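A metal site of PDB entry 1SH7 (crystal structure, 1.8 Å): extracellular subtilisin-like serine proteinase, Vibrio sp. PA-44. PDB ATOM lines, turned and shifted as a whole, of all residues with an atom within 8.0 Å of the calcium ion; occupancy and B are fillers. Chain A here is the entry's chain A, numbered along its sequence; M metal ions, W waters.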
ATOM      1  N   THR A  38      -3.305  -9.509  17.858  1.00  0.00           N
ATOM      2  CA  THR A  38      -2.268  -8.929  18.690  1.00  0.00           C
ATOM      3  C   THR A  38      -2.664  -7.604  19.332  1.00  0.00           C
ATOM      4  O   THR A  38      -1.829  -6.919  19.920  1.00  0.00           O
ATOM      5  CB  THR A  38      -0.964  -8.677  17.848  1.00  0.00           C
ATOM      6  OG1 THR A  38      -1.242  -7.728  16.809  1.00  0.00           O
ATOM      7  CG2 THR A  38      -0.503  -9.910  17.121  1.00  0.00           C
ATOM      8  N   SER A  53     -10.771  -0.398  22.634  1.00  0.00           N
ATOM      9  CA  SER A  53     -10.260  -1.603  23.262  1.00  0.00           C
ATOM     10  C   SER A  53     -11.437  -2.503  23.699  1.00  0.00           C
ATOM     11  O   SER A  53     -12.507  -2.033  24.081  1.00  0.00           O
ATOM     12  CB  SER A  53      -9.386  -1.242  24.472  1.00  0.00           C
ATOM     13  OG  SER A  53      -8.127  -0.714  24.074  1.00  0.00           O
ATOM     14  N   TYR A  55     -10.766  -6.275  25.390  1.00  0.00           N
ATOM     15  CA  TYR A  55     -10.014  -6.765  26.532  1.00  0.00           C
ATOM     16  C   TYR A  55      -8.668  -7.314  26.063  1.00  0.00           C
ATOM     17  O   TYR A  55      -8.526  -7.772  24.920  1.00  0.00           O
ATOM     18  CB  TYR A  55     -10.800  -7.858  27.267  1.00  0.00           C
ATOM     19  CG  TYR A  55     -10.216  -8.131  28.644  1.00  0.00           C
ATOM     20  CD1 TYR A  55     -10.517  -7.304  29.719  1.00  0.00           C
ATOM     21  CD2 TYR A  55      -9.369  -9.204  28.867  1.00  0.00           C
ATOM     22  CE1 TYR A  55      -9.955  -7.510  30.988  1.00  0.00           C
ATOM     23  CE2 TYR A  55      -8.841  -9.470  30.140  1.00  0.00           C
ATOM     24  CZ  TYR A  55      -9.133  -8.625  31.192  1.00  0.00           C
ATOM     25  OH  TYR A  55      -8.551  -8.882  32.436  1.00  0.00           O
ATOM     26  N   ASP A  56      -7.673  -7.256  26.948  1.00  0.00           N
ATOM     27  CA  ASP A  56      -6.323  -7.835  26.707  1.00  0.00           C
ATOM     28  C   ASP A  56      -6.069  -9.083  27.566  1.00  0.00           C
ATOM     29  O   ASP A  56      -5.749  -8.981  28.749  1.00  0.00           O
ATOM     30  CB  ASP A  56      -5.277  -6.729  26.991  1.00  0.00           C
ATOM     31  CG  ASP A  56      -3.844  -7.190  26.822  1.00  0.00           C
ATOM     32  OD1 ASP A  56      -2.924  -6.304  26.892  1.00  0.00           O
ATOM     33  OD2 ASP A  56      -3.523  -8.379  26.635  1.00  0.00           O
ATOM     34  N   PHE A  57      -6.175 -10.260  26.971  1.00  0.00           N
ATOM     35  CA  PHE A  57      -5.974 -11.526  27.673  1.00  0.00           C
ATOM     36  C   PHE A  57      -4.518 -11.993  27.746  1.00  0.00           C
ATOM     37  O   PHE A  57      -4.242 -13.030  28.339  1.00  0.00           O
ATOM     38  CB  PHE A  57      -6.785 -12.639  27.016  1.00  0.00           C
ATOM     39  CG  PHE A  57      -8.251 -12.481  27.229  1.00  0.00           C
ATOM     40  CD1 PHE A  57      -8.818 -12.890  28.426  1.00  0.00           C
ATOM     41  CD2 PHE A  57      -9.030 -11.875  26.266  1.00  0.00           C
ATOM     42  CE1 PHE A  57     -10.179 -12.734  28.636  1.00  0.00           C
ATOM     43  CE2 PHE A  57     -10.385 -11.684  26.465  1.00  0.00           C
ATOM     44  CZ  PHE A  57     -10.956 -12.111  27.656  1.00  0.00           C
ATOM     45  N   VAL A  58      -3.619 -11.266  27.099  1.00  0.00           N
ATOM     46  CA  VAL A  58      -2.202 -11.527  27.200  1.00  0.00           C
ATOM     47  C   VAL A  58      -1.737 -10.952  28.548  1.00  0.00           C
ATOM     48  O   VAL A  58      -1.101 -11.627  29.346  1.00  0.00           O
ATOM     49  CB  VAL A  58      -1.422 -10.863  26.000  1.00  0.00           C
ATOM     50  CG1 VAL A  58       0.078 -10.926  26.190  1.00  0.00           C
ATOM     51  CG2 VAL A  58      -1.802 -11.511  24.675  1.00  0.00           C
ATOM     52  N   ASP A  59      -2.070  -9.706  28.826  1.00  0.00           N
ATOM     53  CA  ASP A  59      -1.604  -9.070  30.063  1.00  0.00           C
ATOM     54  C   ASP A  59      -2.694  -8.859  31.139  1.00  0.00           C
ATOM     55  O   ASP A  59      -2.449  -8.250  32.179  1.00  0.00           O
ATOM     56  CB  ASP A  59      -0.939  -7.738  29.711  1.00  0.00           C
ATOM     57  CG  ASP A  59       0.384  -7.948  29.017  1.00  0.00           C
ATOM     58  OD1 ASP A  59       1.080  -8.925  29.374  1.00  0.00           O
ATOM     59  OD2 ASP A  59       0.791  -7.226  28.085  1.00  0.00           O
ATOM     60  N   ASN A  60      -3.893  -9.376  30.870  1.00  0.00           N
ATOM     61  CA  ASN A  60      -5.051  -9.168  31.728  1.00  0.00           C
ATOM     62  C   ASN A  60      -5.237  -7.716  32.122  1.00  0.00           C
ATOM     63  O   ASN A  60      -5.129  -7.337  33.286  1.00  0.00           O
ATOM     64  CB  ASN A  60      -5.009 -10.115  32.918  1.00  0.00           C
ATOM     65  CG  ASN A  60      -5.094 -11.565  32.491  1.00  0.00           C
ATOM     66  OD1 ASN A  60      -6.014 -11.955  31.748  1.00  0.00           O
ATOM     67  ND2 ASN A  60      -4.094 -12.363  32.876  1.00  0.00           N
ATOM     68  N   ASP A  61      -5.547  -6.896  31.128  1.00  0.00           N
ATOM     69  CA  ASP A  61      -5.777  -5.481  31.323  1.00  0.00           C
ATOM     70  C   ASP A  61      -6.816  -4.982  30.290  1.00  0.00           C
ATOM     71  O   ASP A  61      -7.286  -5.765  29.457  1.00  0.00           O
ATOM     72  CB  ASP A  61      -4.446  -4.705  31.332  1.00  0.00           C
ATOM     73  CG  ASP A  61      -3.781  -4.579  29.977  1.00  0.00           C
ATOM     74  OD1 ASP A  61      -4.418  -4.132  28.997  1.00  0.00           O
ATOM     75  OD2 ASP A  61      -2.568  -4.892  29.818  1.00  0.00           O
ATOM     76  N   ALA A  62      -7.201  -3.722  30.413  1.00  0.00           N
ATOM     77  CA  ALA A  62      -8.316  -3.155  29.631  1.00  0.00           C
ATOM     78  C   ALA A  62      -7.889  -2.472  28.342  1.00  0.00           C
ATOM     79  O   ALA A  62      -8.740  -1.909  27.636  1.00  0.00           O
ATOM     80  CB  ALA A  62      -9.127  -2.151  30.501  1.00  0.00           C
ATOM     81  N   ASP A  63      -6.592  -2.494  28.049  1.00  0.00           N
ATOM     82  CA  ASP A  63      -6.022  -1.750  26.946  1.00  0.00           C
ATOM     83  C   ASP A  63      -5.460  -2.748  25.927  1.00  0.00           C
ATOM     84  O   ASP A  63      -4.418  -3.378  26.153  1.00  0.00           O
ATOM     85  CB  ASP A  63      -4.945  -0.780  27.463  1.00  0.00           C
ATOM     86  CG  ASP A  63      -4.359   0.090  26.364  1.00  0.00           C
ATOM     87  OD1 ASP A  63      -3.701   1.117  26.672  1.00  0.00           O
ATOM     88  OD2 ASP A  63      -4.543  -0.184  25.173  1.00  0.00           O
ATOM     89  N   SER A  64      -6.189  -2.913  24.830  1.00  0.00           N
ATOM     90  CA  SER A  64      -5.848  -3.891  23.781  1.00  0.00           C
ATOM     91  C   SER A  64      -4.984  -3.278  22.695  1.00  0.00           C
ATOM     92  O   SER A  64      -5.012  -3.741  21.527  1.00  0.00           O
ATOM     93  CB  SER A  64      -7.097  -4.531  23.195  1.00  0.00           C
ATOM     94  OG  SER A  64      -8.056  -3.590  22.781  1.00  0.00           O
ATOM     95  N   SER A  65      -4.170  -2.299  23.061  1.00  0.00           N
ATOM     96  CA  SER A  65      -3.166  -1.725  22.137  1.00  0.00           C
ATOM     97  C   SER A  65      -2.276  -2.822  21.557  1.00  0.00           C
ATOM     98  O   SER A  65      -2.049  -3.827  22.185  1.00  0.00           O
ATOM     99  CB  SER A  65      -2.296  -0.694  22.831  1.00  0.00           C
ATOM    100  OG  SER A  65      -3.021   0.487  23.129  1.00  0.00           O
ATOM    101  N   ASP A  66      -1.807  -2.605  20.322  1.00  0.00           N
ATOM    102  CA  ASP A  66      -1.071  -3.550  19.519  1.00  0.00           C
ATOM    103  C   ASP A  66       0.423  -3.179  19.601  1.00  0.00           C
ATOM    104  O   ASP A  66       0.779  -2.048  19.289  1.00  0.00           O
ATOM    105  CB  ASP A  66      -1.540  -3.403  18.081  1.00  0.00           C
ATOM    106  CG  ASP A  66      -0.865  -4.370  17.110  1.00  0.00           C
ATOM    107  OD1 ASP A  66      -0.171  -5.338  17.537  1.00  0.00           O
ATOM    108  OD2 ASP A  66      -0.991  -4.215  15.873  1.00  0.00           O
ATOM    109  N   CYS A  67       1.272  -4.133  19.976  1.00  0.00           N
ATOM    110  CA  CYS A  67       2.750  -3.961  20.017  1.00  0.00           C
ATOM    111  C   CYS A  67       3.503  -4.925  19.075  1.00  0.00           C
ATOM    112  O   CYS A  67       4.713  -5.152  19.223  1.00  0.00           O
ATOM    113  CB  CYS A  67       3.261  -4.072  21.446  1.00  0.00           C
ATOM    114  SG  CYS A  67       2.747  -5.571  22.276  1.00  0.00           S
ATOM    115  N   ARG A  95      -7.201  -8.669  22.367  1.00  0.00           N
ATOM    116  CA  ARG A  95      -5.812  -9.032  22.316  1.00  0.00           C
ATOM    117  C   ARG A  95      -5.526 -10.397  22.966  1.00  0.00           C
ATOM    118  O   ARG A  95      -5.608 -10.552  24.193  1.00  0.00           O
ATOM    119  CB  ARG A  95      -4.955  -7.929  22.914  1.00  0.00           C
ATOM    120  CG  ARG A  95      -3.450  -8.229  22.913  1.00  0.00           C
ATOM    121  CD  ARG A  95      -2.630  -7.045  23.342  1.00  0.00           C
ATOM    122  NE  ARG A  95      -1.212  -7.314  23.166  1.00  0.00           N
ATOM    123  CZ  ARG A  95      -0.317  -7.520  24.121  1.00  0.00           C
ATOM    124  NH1 ARG A  95       0.936  -7.770  23.762  1.00  0.00           N
ATOM    125  NH2 ARG A  95      -0.588  -7.430  25.401  1.00  0.00           N
HETATM  126 CA    CA M   1      -2.542  -4.155  27.273  1.00  0.00          CA
HETATM  127  O   HOH W   1      -1.835  -1.979  27.901  1.00  0.00           O
HETATM  128  O   HOH W   2      -1.690  -3.981  25.061  1.00  0.00           O
HETATM  129  O   HOH W   3      -0.236  -4.837  27.637  1.00  0.00           O
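The guanidinium group of Arg 95 lies within salt-bridge range of the side-chain carboxylate of Asp 56 (3.3 Å).
OD2 of Asp 56 sits at hydrogen-bond distance from N of Asp 59.
The side-chain carboxylate (OD2) of Asp 56 is in hydrogen-bond range of the backbone NH (N) of Val 58 (2.9 Å).
OG of Ser 65 is in hydrogen-bond range of OD2 of Asp 63 (2.6 Å).
Within 4 Å of the calcium ion: Asp 56, Asp 61 and Asp 63.
The calcium ion is bound by OD1 of Asp 56 (2.2 Å).
O of Asp 63 is bound to the calcium ion.
Water W1 is bound to the calcium ion (2.4 Å).
The calcium ion is bound by water W2, at 2.4 Å.
Water W3 binds the calcium ion, at 2.4 Å.
The side-chain carboxylate (OD1) of Asp 61 is bound to the calcium ion (2.5 Å).
OD2 of Asp 61 is bound to the calcium ion (2.6 Å).
The calcium ion has seven donor atoms within binding distance.
Water W3 bridges the side-chain carboxylate (OD2) of Asp 59 (2.6 Å) and the guanidinium group (NH2) of Arg 95 (3.4 Å).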
